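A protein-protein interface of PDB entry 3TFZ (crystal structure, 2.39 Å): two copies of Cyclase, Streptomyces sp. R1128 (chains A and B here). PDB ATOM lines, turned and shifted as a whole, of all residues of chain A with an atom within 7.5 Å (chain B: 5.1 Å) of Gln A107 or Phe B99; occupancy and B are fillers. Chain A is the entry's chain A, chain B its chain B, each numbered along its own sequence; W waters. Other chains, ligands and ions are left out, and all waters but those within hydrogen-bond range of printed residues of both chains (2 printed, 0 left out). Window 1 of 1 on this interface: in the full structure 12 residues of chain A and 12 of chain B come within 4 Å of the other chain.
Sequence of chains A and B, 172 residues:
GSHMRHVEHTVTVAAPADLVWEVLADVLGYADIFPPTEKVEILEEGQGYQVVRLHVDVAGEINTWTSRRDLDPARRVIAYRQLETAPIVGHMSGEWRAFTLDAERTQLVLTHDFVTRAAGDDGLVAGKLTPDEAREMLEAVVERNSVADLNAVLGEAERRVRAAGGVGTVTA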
ATOM      1  N   HIS A   9     -18.864  -9.319  -1.269  1.00  0.00           N
ATOM      2  CA  HIS A   9     -18.999  -7.846  -1.263  1.00  0.00           C
ATOM      3  C   HIS A   9     -18.193  -7.344  -2.458  1.00  0.00           C
ATOM      4  O   HIS A   9     -17.274  -8.044  -2.861  1.00  0.00           O
ATOM      5  CB  HIS A   9     -18.495  -7.178   0.014  1.00  0.00           C
ATOM      6  CG  HIS A   9     -19.297  -7.506   1.240  1.00  0.00           C
ATOM      7  ND1 HIS A   9     -19.226  -8.734   1.883  1.00  0.00           N
ATOM      8  CD2 HIS A   9     -20.160  -6.761   1.967  1.00  0.00           C
ATOM      9  CE1 HIS A   9     -20.003  -8.726   2.952  1.00  0.00           C
ATOM     10  NE2 HIS A   9     -20.578  -7.540   3.024  1.00  0.00           N
ATOM     11  N   THR A  10     -18.508  -6.147  -2.965  1.00  0.00           N
ATOM     12  CA  THR A  10     -17.800  -5.643  -4.125  1.00  0.00           C
ATOM     13  C   THR A  10     -17.732  -4.129  -4.091  1.00  0.00           C
ATOM     14  O   THR A  10     -18.555  -3.495  -3.417  1.00  0.00           O
ATOM     15  CB  THR A  10     -18.414  -6.220  -5.501  1.00  0.00           C
ATOM     16  OG1 THR A  10     -17.558  -5.968  -6.582  1.00  0.00           O
ATOM     17  CG2 THR A  10     -19.885  -5.733  -5.826  1.00  0.00           C
ATOM     18  N   VAL A  11     -16.780  -3.601  -4.871  1.00  0.00           N
ATOM     19  CA  VAL A  11     -16.528  -2.158  -5.138  1.00  0.00           C
ATOM     20  C   VAL A  11     -15.912  -2.085  -6.553  1.00  0.00           C
ATOM     21  O   VAL A  11     -15.340  -3.095  -7.038  1.00  0.00           O
ATOM     22  CB  VAL A  11     -15.603  -1.737  -3.982  1.00  0.00           C
ATOM     23  CG1 VAL A  11     -14.019  -1.853  -4.157  1.00  0.00           C
ATOM     24  CG2 VAL A  11     -16.297  -0.950  -2.828  1.00  0.00           C
ATOM     25  N   THR A  12     -16.124  -0.946  -7.245  1.00  0.00           N
ATOM     26  CA  THR A  12     -15.647  -0.647  -8.579  1.00  0.00           C
ATOM     27  C   THR A  12     -14.469   0.227  -8.320  1.00  0.00           C
ATOM     28  O   THR A  12     -14.636   1.262  -7.687  1.00  0.00           O
ATOM     29  CB  THR A  12     -16.735   0.113  -9.393  1.00  0.00           C
ATOM     30  OG1 THR A  12     -17.810  -0.765  -9.657  1.00  0.00           O
ATOM     31  CG2 THR A  12     -16.241   0.479 -10.752  1.00  0.00           C
ATOM     32  N   VAL A  13     -13.272  -0.159  -8.781  1.00  0.00           N
ATOM     33  CA  VAL A  13     -12.013   0.619  -8.549  1.00  0.00           C
ATOM     34  C   VAL A  13     -11.652   1.452  -9.790  1.00  0.00           C
ATOM     35  O   VAL A  13     -11.613   0.930 -10.930  1.00  0.00           O
ATOM     36  CB  VAL A  13     -10.859  -0.285  -8.159  1.00  0.00           C
ATOM     37  CG1 VAL A  13      -9.520   0.542  -7.740  1.00  0.00           C
ATOM     38  CG2 VAL A  13     -11.296  -1.196  -6.947  1.00  0.00           C
ATOM     39  N   ALA A  15      -9.152   2.162 -11.371  1.00  0.00           N
ATOM     40  CA  ALA A  15      -7.725   1.861 -11.731  1.00  0.00           C
ATOM     41  C   ALA A  15      -7.743   0.637 -12.622  1.00  0.00           C
ATOM     42  O   ALA A  15      -8.663  -0.209 -12.488  1.00  0.00           O
ATOM     43  CB  ALA A  15      -6.853   1.556 -10.467  1.00  0.00           C
ATOM     44  N   ALA A  17      -6.816  -3.271 -13.970  1.00  0.00           N
ATOM     45  CA  ALA A  17      -6.933  -4.507 -13.177  1.00  0.00           C
ATOM     46  C   ALA A  17      -5.570  -4.975 -12.766  1.00  0.00           C
ATOM     47  O   ALA A  17      -5.417  -5.476 -11.700  1.00  0.00           O
ATOM     48  CB  ALA A  17      -7.736  -5.569 -13.960  1.00  0.00           C
ATOM     49  N   VAL A  20      -4.495  -3.039  -9.639  1.00  0.00           N
ATOM     50  CA  VAL A  20      -5.195  -3.607  -8.518  1.00  0.00           C
ATOM     51  C   VAL A  20      -4.565  -4.927  -8.107  1.00  0.00           C
ATOM     52  O   VAL A  20      -4.514  -5.221  -6.960  1.00  0.00           O
ATOM     53  CB  VAL A  20      -6.673  -3.780  -8.868  1.00  0.00           C
ATOM     54  CG1 VAL A  20      -7.417  -4.469  -7.744  1.00  0.00           C
ATOM     55  CG2 VAL A  20      -7.329  -2.409  -9.171  1.00  0.00           C
ATOM     56  N   ARG A  76      -6.466 -13.583 -12.023  1.00  0.00           N
ATOM     57  CA  ARG A  76      -6.653 -12.427 -11.089  1.00  0.00           C
ATOM     58  C   ARG A  76      -7.505 -12.764  -9.840  1.00  0.00           C
ATOM     59  O   ARG A  76      -8.515 -12.070  -9.535  1.00  0.00           O
ATOM     60  CB  ARG A  76      -7.196 -11.154 -11.723  1.00  0.00           C
ATOM     61  CG  ARG A  76      -6.709 -10.788 -13.088  1.00  0.00           C
ATOM     62  CD  ARG A  76      -7.622  -9.633 -13.649  1.00  0.00           C
ATOM     63  NE  ARG A  76      -7.219  -9.227 -14.970  1.00  0.00           N
ATOM     64  CZ  ARG A  76      -6.102  -8.571 -15.235  1.00  0.00           C
ATOM     65  NH1 ARG A  76      -5.279  -8.287 -14.268  1.00  0.00           N
ATOM     66  NH2 ARG A  76      -5.827  -8.188 -16.463  1.00  0.00           N
ATOM     67  N   ARG A  97     -11.158 -11.406  -6.120  1.00  0.00           N
ATOM     68  CA  ARG A  97     -11.296 -11.499  -7.543  1.00  0.00           C
ATOM     69  C   ARG A  97     -11.397 -10.061  -8.118  1.00  0.00           C
ATOM     70  O   ARG A  97     -12.279  -9.327  -7.755  1.00  0.00           O
ATOM     71  CB  ARG A  97     -12.580 -12.229  -7.902  1.00  0.00           C
ATOM     72  CG  ARG A  97     -12.805 -13.643  -7.199  1.00  0.00           C
ATOM     73  CD  ARG A  97     -14.321 -13.990  -7.221  1.00  0.00           C
ATOM     74  NE  ARG A  97     -14.557 -15.314  -6.651  1.00  0.00           N
ATOM     75  CZ  ARG A  97     -15.735 -15.899  -6.499  1.00  0.00           C
ATOM     76  NH1 ARG A  97     -16.839 -15.295  -6.892  1.00  0.00           N
ATOM     77  NH2 ARG A  97     -15.811 -17.118  -5.977  1.00  0.00           N
ATOM     78  N   ALA A  98     -10.542  -9.727  -9.104  1.00  0.00           N
ATOM     79  CA  ALA A  98     -10.453  -8.468  -9.782  1.00  0.00           C
ATOM     80  C   ALA A  98     -10.880  -8.696 -11.230  1.00  0.00           C
ATOM     81  O   ALA A  98     -10.231  -9.416 -11.884  1.00  0.00           O
ATOM     82  CB  ALA A  98      -9.009  -7.997  -9.767  1.00  0.00           C
ATOM     83  N   PHE A  99     -11.929  -8.087 -11.750  1.00  0.00           N
ATOM     84  CA  PHE A  99     -12.328  -8.243 -13.112  1.00  0.00           C
ATOM     85  C   PHE A  99     -12.054  -6.928 -13.881  1.00  0.00           C
ATOM     86  O   PHE A  99     -12.276  -5.850 -13.360  1.00  0.00           O
ATOM     87  CB  PHE A  99     -13.791  -8.553 -13.162  1.00  0.00           C
ATOM     88  CG  PHE A  99     -14.183  -9.845 -12.423  1.00  0.00           C
ATOM     89  CD1 PHE A  99     -14.282 -11.020 -13.103  1.00  0.00           C
ATOM     90  CD2 PHE A  99     -14.627  -9.819 -11.097  1.00  0.00           C
ATOM     91  CE1 PHE A  99     -14.647 -12.160 -12.442  1.00  0.00           C
ATOM     92  CE2 PHE A  99     -15.003 -10.884 -10.487  1.00  0.00           C
ATOM     93  CZ  PHE A  99     -15.036 -12.110 -11.182  1.00  0.00           C
ATOM     94  N   THR A 100     -11.466  -7.028 -15.084  1.00  0.00           N
ATOM     95  CA  THR A 100     -11.479  -5.942 -16.040  1.00  0.00           C
ATOM     96  C   THR A 100     -12.932  -5.534 -16.380  1.00  0.00           C
ATOM     97  O   THR A 100     -13.749  -6.386 -16.915  1.00  0.00           O
ATOM     98  CB  THR A 100     -10.790  -6.428 -17.335  1.00  0.00           C
ATOM     99  OG1 THR A 100      -9.401  -6.602 -17.031  1.00  0.00           O
ATOM    100  CG2 THR A 100     -10.909  -5.436 -18.351  1.00  0.00           C
ATOM    101  N   LEU A 101     -13.264  -4.276 -16.061  1.00  0.00           N
ATOM    102  CA  LEU A 101     -14.532  -3.689 -16.417  1.00  0.00           C
ATOM    103  C   LEU A 101     -14.272  -2.886 -17.706  1.00  0.00           C
ATOM    104  O   LEU A 101     -14.913  -3.098 -18.754  1.00  0.00           O
ATOM    105  CB  LEU A 101     -15.037  -2.820 -15.249  1.00  0.00           C
ATOM    106  CG  LEU A 101     -16.371  -2.048 -15.413  1.00  0.00           C
ATOM    107  CD1 LEU A 101     -17.591  -2.910 -15.855  1.00  0.00           C
ATOM    108  CD2 LEU A 101     -16.684  -1.390 -14.126  1.00  0.00           C
ATOM    109  N   ASP A 102     -13.296  -1.988 -17.678  1.00  0.00           N
ATOM    110  CA  ASP A 102     -12.723  -1.571 -18.916  1.00  0.00           C
ATOM    111  C   ASP A 102     -11.229  -1.310 -18.704  1.00  0.00           C
ATOM    112  O   ASP A 102     -10.670  -1.705 -17.677  1.00  0.00           O
ATOM    113  CB  ASP A 102     -13.535  -0.392 -19.482  1.00  0.00           C
ATOM    114  CG  ASP A 102     -13.476   0.849 -18.591  1.00  0.00           C
ATOM    115  OD1 ASP A 102     -14.480   1.588 -18.403  1.00  0.00           O
ATOM    116  OD2 ASP A 102     -12.391   1.069 -18.049  1.00  0.00           O
ATOM    117  N   ARG A 105     -11.069   0.698 -15.424  1.00  0.00           N
ATOM    118  CA  ARG A 105     -11.847   0.357 -14.235  1.00  0.00           C
ATOM    119  C   ARG A 105     -11.830  -1.107 -13.971  1.00  0.00           C
ATOM    120  O   ARG A 105     -11.640  -1.890 -14.900  1.00  0.00           O
ATOM    121  CB  ARG A 105     -13.277   0.864 -14.288  1.00  0.00           C
ATOM    122  CG  ARG A 105     -13.342   2.363 -14.511  1.00  0.00           C
ATOM    123  CD  ARG A 105     -14.811   2.762 -14.640  1.00  0.00           C
ATOM    124  NE  ARG A 105     -15.413   2.244 -15.862  1.00  0.00           N
ATOM    125  CZ  ARG A 105     -16.720   2.039 -15.988  1.00  0.00           C
ATOM    126  NH1 ARG A 105     -17.518   2.254 -14.942  1.00  0.00           N
ATOM    127  NH2 ARG A 105     -17.207   1.548 -17.126  1.00  0.00           N
ATOM    128  N   THR A 106     -11.971  -1.480 -12.689  1.00  0.00           N
ATOM    129  CA  THR A 106     -11.827  -2.869 -12.302  1.00  0.00           C
ATOM    130  C   THR A 106     -12.997  -3.113 -11.364  1.00  0.00           C
ATOM    131  O   THR A 106     -13.255  -2.343 -10.481  1.00  0.00           O
ATOM    132  CB  THR A 106     -10.479  -3.039 -11.532  1.00  0.00           C
ATOM    133  OG1 THR A 106      -9.411  -2.750 -12.375  1.00  0.00           O
ATOM    134  CG2 THR A 106     -10.195  -4.413 -10.982  1.00  0.00           C
ATOM    135  N   GLN A 107     -13.676  -4.235 -11.503  1.00  0.00           N
ATOM    136  CA  GLN A 107     -14.603  -4.681 -10.465  1.00  0.00           C
ATOM    137  C   GLN A 107     -13.791  -5.518  -9.427  1.00  0.00           C
ATOM    138  O   GLN A 107     -13.113  -6.495  -9.786  1.00  0.00           O
ATOM    139  CB  GLN A 107     -15.682  -5.563 -11.103  1.00  0.00           C
ATOM    140  CG  GLN A 107     -16.936  -5.871 -10.225  1.00  0.00           C
ATOM    141  CD  GLN A 107     -17.813  -4.679 -10.105  1.00  0.00           C
ATOM    142  OE1 GLN A 107     -18.298  -4.115 -11.086  1.00  0.00           O
ATOM    143  NE2 GLN A 107     -18.030  -4.255  -8.879  1.00  0.00           N
ATOM    144  N   LEU A 108     -13.910  -5.156  -8.155  1.00  0.00           N
ATOM    145  CA  LEU A 108     -13.153  -5.809  -7.082  1.00  0.00           C
ATOM    146  C   LEU A 108     -14.136  -6.596  -6.143  1.00  0.00           C
ATOM    147  O   LEU A 108     -15.065  -6.042  -5.575  1.00  0.00           O
ATOM    148  CB  LEU A 108     -12.265  -4.783  -6.271  1.00  0.00           C
ATOM    149  CG  LEU A 108     -11.411  -5.460  -5.174  1.00  0.00           C
ATOM    150  CD1 LEU A 108     -10.334  -6.485  -5.750  1.00  0.00           C
ATOM    151  CD2 LEU A 108     -10.666  -4.426  -4.364  1.00  0.00           C
ATOM    152  N   VAL A 109     -13.885  -7.887  -6.009  1.00  0.00           N
ATOM    153  CA  VAL A 109     -14.654  -8.763  -5.196  1.00  0.00           C
ATOM    154  C   VAL A 109     -13.842  -9.501  -4.092  1.00  0.00           C
ATOM    155  O   VAL A 109     -12.744 -10.004  -4.313  1.00  0.00           O
ATOM    156  CB  VAL A 109     -15.397  -9.812  -6.083  1.00  0.00           C
ATOM    157  CG1 VAL A 109     -16.330 -10.741  -5.203  1.00  0.00           C
ATOM    158  CG2 VAL A 109     -16.242  -9.084  -7.136  1.00  0.00           C
ATOM    159  N   LEU A 150     -11.948  -3.956   1.233  1.00  0.00           N
ATOM    160  CA  LEU A 150     -12.326  -3.497  -0.121  1.00  0.00           C
ATOM    161  C   LEU A 150     -11.982  -2.034  -0.342  1.00  0.00           C
ATOM    162  O   LEU A 150     -11.405  -1.758  -1.346  1.00  0.00           O
ATOM    163  CB  LEU A 150     -13.826  -3.761  -0.386  1.00  0.00           C
ATOM    164  CG  LEU A 150     -14.242  -5.191  -0.791  1.00  0.00           C
ATOM    165  CD1 LEU A 150     -15.768  -5.390  -0.785  1.00  0.00           C
ATOM    166  CD2 LEU A 150     -13.693  -5.648  -2.199  1.00  0.00           C
ATOM    167  N   GLU B   8     -23.085  -1.167  -4.183  1.00  0.00           N
ATOM    168  CA  GLU B   8     -22.995  -2.269  -5.117  1.00  0.00           C
ATOM    169  C   GLU B   8     -23.229  -3.541  -4.348  1.00  0.00           C
ATOM    170  O   GLU B   8     -22.772  -3.665  -3.220  1.00  0.00           O
ATOM    171  CB  GLU B   8     -21.611  -2.379  -5.783  1.00  0.00           C
ATOM    172  CG  GLU B   8     -20.899  -1.104  -5.920  1.00  0.00           C
ATOM    173  CD  GLU B   8     -19.877  -1.092  -7.026  1.00  0.00           C
ATOM    174  OE1 GLU B   8     -19.603  -2.192  -7.531  1.00  0.00           O
ATOM    175  OE2 GLU B   8     -19.316   0.021  -7.338  1.00  0.00           O
ATOM    176  N   ALA B  17     -22.202 -16.929 -18.265  1.00  0.00           N
ATOM    177  CA  ALA B  17     -22.492 -15.489 -18.375  1.00  0.00           C
ATOM    178  C   ALA B  17     -23.498 -15.162 -19.497  1.00  0.00           C
ATOM    179  O   ALA B  17     -24.321 -14.270 -19.314  1.00  0.00           O
ATOM    180  CB  ALA B  17     -21.220 -14.722 -18.571  1.00  0.00           C
ATOM    181  N   ARG B  97     -23.949  -5.822 -14.379  1.00  0.00           N
ATOM    182  CA  ARG B  97     -22.786  -6.367 -15.033  1.00  0.00           C
ATOM    183  C   ARG B  97     -22.692  -7.844 -14.762  1.00  0.00           C
ATOM    184  O   ARG B  97     -22.749  -8.289 -13.598  1.00  0.00           O
ATOM    185  CB  ARG B  97     -21.588  -5.708 -14.399  1.00  0.00           C
ATOM    186  CG  ARG B  97     -21.720  -4.185 -14.325  1.00  0.00           C
ATOM    187  CD  ARG B  97     -20.762  -3.546 -13.413  1.00  0.00           C
ATOM    188  NE  ARG B  97     -20.767  -2.056 -13.563  1.00  0.00           N
ATOM    189  CZ  ARG B  97     -20.202  -1.234 -12.696  1.00  0.00           C
ATOM    190  NH1 ARG B  97     -19.570  -1.768 -11.616  1.00  0.00           N
ATOM    191  NH2 ARG B  97     -20.221   0.103 -12.931  1.00  0.00           N
ATOM    192  N   ALA B  98     -22.490  -8.635 -15.825  1.00  0.00           N
ATOM    193  CA  ALA B  98     -22.279 -10.107 -15.714  1.00  0.00           C
ATOM    194  C   ALA B  98     -20.798 -10.372 -16.126  1.00  0.00           C
ATOM    195  O   ALA B  98     -20.517 -10.280 -17.308  1.00  0.00           O
ATOM    196  CB  ALA B  98     -23.242 -10.867 -16.661  1.00  0.00           C
ATOM    197  N   PHE B  99     -19.888 -10.723 -15.201  1.00  0.00           N
ATOM    198  CA  PHE B  99     -18.552 -11.091 -15.594  1.00  0.00           C
ATOM    199  C   PHE B  99     -18.361 -12.569 -15.706  1.00  0.00           C
ATOM    200  O   PHE B  99     -18.990 -13.311 -14.986  1.00  0.00           O
ATOM    201  CB  PHE B  99     -17.553 -10.586 -14.563  1.00  0.00           C
ATOM    202  CG  PHE B  99     -17.557  -9.082 -14.390  1.00  0.00           C
ATOM    203  CD1 PHE B  99     -16.845  -8.286 -15.257  1.00  0.00           C
ATOM    204  CD2 PHE B  99     -18.345  -8.469 -13.390  1.00  0.00           C
ATOM    205  CE1 PHE B  99     -16.781  -6.876 -15.067  1.00  0.00           C
ATOM    206  CE2 PHE B  99     -18.356  -7.097 -13.268  1.00  0.00           C
ATOM    207  CZ  PHE B  99     -17.558  -6.289 -14.083  1.00  0.00           C
ATOM    208  N   THR B 100     -17.452 -13.012 -16.575  1.00  0.00           N
ATOM    209  CA  THR B 100     -17.105 -14.419 -16.677  1.00  0.00           C
ATOM    210  C   THR B 100     -16.174 -14.821 -15.511  1.00  0.00           C
ATOM    211  O   THR B 100     -15.075 -14.279 -15.359  1.00  0.00           O
ATOM    212  CB  THR B 100     -16.394 -14.736 -18.065  1.00  0.00           C
ATOM    213  OG1 THR B 100     -17.414 -14.820 -19.082  1.00  0.00           O
ATOM    214  CG2 THR B 100     -15.592 -16.128 -17.984  1.00  0.00           C
ATOM    215  N   LEU B 101     -16.594 -15.785 -14.719  1.00  0.00           N
ATOM    216  CA  LEU B 101     -15.709 -16.363 -13.711  1.00  0.00           C
ATOM    217  C   LEU B 101     -14.994 -17.673 -14.246  1.00  0.00           C
ATOM    218  O   LEU B 101     -13.778 -17.882 -14.075  1.00  0.00           O
ATOM    219  CB  LEU B 101     -16.553 -16.592 -12.468  1.00  0.00           C
ATOM    220  CG  LEU B 101     -16.055 -16.844 -11.061  1.00  0.00           C
ATOM    221  CD1 LEU B 101     -15.002 -15.922 -10.565  1.00  0.00           C
ATOM    222  CD2 LEU B 101     -17.358 -16.622 -10.366  1.00  0.00           C
ATOM    223  N   ARG B 105     -19.732 -20.239 -14.622  1.00  0.00           N
ATOM    224  CA  ARG B 105     -20.120 -19.418 -13.449  1.00  0.00           C
ATOM    225  C   ARG B 105     -19.961 -17.976 -13.786  1.00  0.00           C
ATOM    226  O   ARG B 105     -19.039 -17.574 -14.533  1.00  0.00           O
ATOM    227  CB  ARG B 105     -19.284 -19.776 -12.183  1.00  0.00           C
ATOM    228  CG  ARG B 105     -19.648 -21.143 -11.559  1.00  0.00           C
ATOM    229  CD  ARG B 105     -18.872 -21.412 -10.276  1.00  0.00           C
ATOM    230  NE  ARG B 105     -17.435 -21.097 -10.441  1.00  0.00           N
ATOM    231  CZ  ARG B 105     -16.580 -20.728  -9.455  1.00  0.00           C
ATOM    232  NH1 ARG B 105     -16.969 -20.549  -8.196  1.00  0.00           N
ATOM    233  NH2 ARG B 105     -15.304 -20.511  -9.754  1.00  0.00           N
ATOM    234  N   THR B 106     -20.837 -17.162 -13.224  1.00  0.00           N
ATOM    235  CA  THR B 106     -20.861 -15.695 -13.492  1.00  0.00           C
ATOM    236  C   THR B 106     -20.762 -14.933 -12.173  1.00  0.00           C
ATOM    237  O   THR B 106     -21.447 -15.286 -11.234  1.00  0.00           O
ATOM    238  CB  THR B 106     -22.213 -15.414 -14.142  1.00  0.00           C
ATOM    239  OG1 THR B 106     -22.300 -16.268 -15.258  1.00  0.00           O
ATOM    240  CG2 THR B 106     -22.438 -13.969 -14.625  1.00  0.00           C
ATOM    241  N   GLN B 107     -19.884 -13.917 -12.104  1.00  0.00           N
ATOM    242  CA  GLN B 107     -19.964 -12.904 -11.091  1.00  0.00           C
ATOM    243  C   GLN B 107     -21.012 -11.868 -11.502  1.00  0.00           C
ATOM    244  O   GLN B 107     -20.790 -11.158 -12.462  1.00  0.00           O
ATOM    245  CB  GLN B 107     -18.623 -12.160 -10.889  1.00  0.00           C
ATOM    246  CG  GLN B 107     -18.633 -11.349  -9.615  1.00  0.00           C
ATOM    247  CD  GLN B 107     -18.415 -12.229  -8.387  1.00  0.00           C
ATOM    248  OE1 GLN B 107     -17.474 -13.002  -8.346  1.00  0.00           O
ATOM    249  NE2 GLN B 107     -19.287 -12.109  -7.380  1.00  0.00           N
ATOM    250  N   LEU B 108     -22.150 -11.809 -10.794  1.00  0.00           N
ATOM    251  CA  LEU B 108     -23.217 -10.886 -11.123  1.00  0.00           C
ATOM    252  C   LEU B 108     -23.261  -9.698 -10.152  1.00  0.00           C
ATOM    253  O   LEU B 108     -23.260  -9.899  -8.954  1.00  0.00           O
ATOM    254  CB  LEU B 108     -24.538 -11.630 -11.248  1.00  0.00           C
ATOM    255  CG  LEU B 108     -25.795 -10.816 -11.544  1.00  0.00           C
ATOM    256  CD1 LEU B 108     -25.794 -10.223 -12.929  1.00  0.00           C
ATOM    257  CD2 LEU B 108     -27.009 -11.704 -11.286  1.00  0.00           C
ATOM    258  N   VAL B 109     -23.176  -8.468 -10.730  1.00  0.00           N
ATOM    259  CA  VAL B 109     -23.158  -7.194 -10.036  1.00  0.00           C
ATOM    260  C   VAL B 109     -24.348  -6.324 -10.412  1.00  0.00           C
ATOM    261  O   VAL B 109     -24.698  -6.189 -11.591  1.00  0.00           O
ATOM    262  CB  VAL B 109     -21.840  -6.441 -10.319  1.00  0.00           C
ATOM    263  CG1 VAL B 109     -21.850  -5.206  -9.550  1.00  0.00           C
ATOM    264  CG2 VAL B 109     -20.638  -7.305  -9.889  1.00  0.00           C
HETATM  265  O   HOH W   1     -21.021  -5.134  -1.872  1.00  0.00           O
HETATM  266  O   HOH W   2     -17.361   1.403  -5.968  1.00  0.00           O
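Water W1 bridges O of Glu B8 (2.7 Å) and N of Thr A10 (2.9 Å). Water W2 lies within hydrogen-bond range of the side-chain carboxylate of Glu B8 (2.8 Å) and the backbone NH of Thr A12 (2.9 Å).
OG1 of Thr A12 is in hydrogen-bond range of OE2 of Glu B8 (2.9 Å). The guanidinium group of Arg B97 sits at hydrogen-bond distance from the side-chain hydroxyl of Thr A12 (2.8 Å). OE1 of Gln B107 sits at hydrogen-bond distance from NH1 of Arg A97 (2.8 Å). The side-chain amide nitrogen of Gln A107 sits at hydrogen-bond distance from the side-chain carboxylate of Glu B8 (2.9 Å). The side-chain amide oxygen (OE1) of Gln A107 is in hydrogen-bond range of the guanidinium group (NH1) of Arg B97 (2.7 Å).
CG2 of Thr A10 touches CB of Glu B8, 3.8 Å away. C of Val A11 touches OE1 of Glu B8 (3.8 Å). Leu B101 touches Arg A97. CB of Phe B99 touches CD1 of Phe A99, 3.6 Å away. Phe A99 touches Thr B100. CE1 of Phe B99 touches O of Thr A100, at 3.6 Å. Arg B97 touches Arg A105 (NH2 to NH1, 3.997 Å). Gln A107 touches Phe B99 (CG to CE2, 3.6 Å). CD of Gln A107 touches CG2 of Val B109 (3.9 Å). Val A109 touches Gln B107 (CG1 to NE2, 3.9 Å).
Hydrophobic or aromatic side chains of chain A within 4 Å of the printed part of chain B: Phe A99, Leu A101 and Val A109. Among the printed residues, 19 pairs touch across the chains.
Of the printed residues of chain B, Gln A107 touches Glu B8, Arg B97, Phe B99 and Val B109. Of the printed residues of chain A, Phe B99 touches Phe A99, Thr A100, Leu A101 and Gln A107. Of the printed residues of chain A, Arg B97 touches Thr A12, Leu A101, Arg A105 and Gln A107. Of the printed residues of chain B, Arg A97 touches Leu B101 and Gln B107. Of the printed residues of chain A, Thr B100 touches Phe A99 (3.6 Å). The nearest printed residue of chain B that does not touch Leu A101 is Glu B8 (7.3 Å).
Phe B99 touches its own counterpart, Phe A99. Phe A99 touches Thr B100, and with the chains exchanged Thr A100 touches Phe B99. Phe A99 touches Gln B107, and with the chains exchanged Gln A107 touches Phe B99. Arg A105 touches Arg B97, but with the chains exchanged Arg A97 does not touch Arg B105 (4.2 Å). Positions printed for both chains: 17, 97, 98, 99, 100, 101, 105, 106, 107, 108 and 109. Of the 19 pairs that touch across the chains among the printed residues, 13 have their exchanged pair printed and touching as well.
OG1 of Thr A10 lies within hydrogen-bond range of NE2 of Gln A107 (2.9 Å). The side-chain hydroxyl (OG1) of Thr A10 is in hydrogen-bond range of the backbone carbonyl oxygen (O) of Leu A108 (2.7 Å). The backbone carbonyl oxygen (O) of Val A11 lies within hydrogen-bond range of the side-chain amide nitrogen (NE2) of Gln A107, 3.5 Å away. O of Val A11 is in hydrogen-bond range of N of Leu A108 (2.7 Å). The backbone NH (N) of Val A109 lies within hydrogen-bond range of the backbone carbonyl oxygen (O) of Arg A97 (2.8 Å). The backbone carbonyl oxygen (O) of Gln B107 sits at hydrogen-bond distance from the backbone NH (N) of Phe B99 (2.9 Å).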
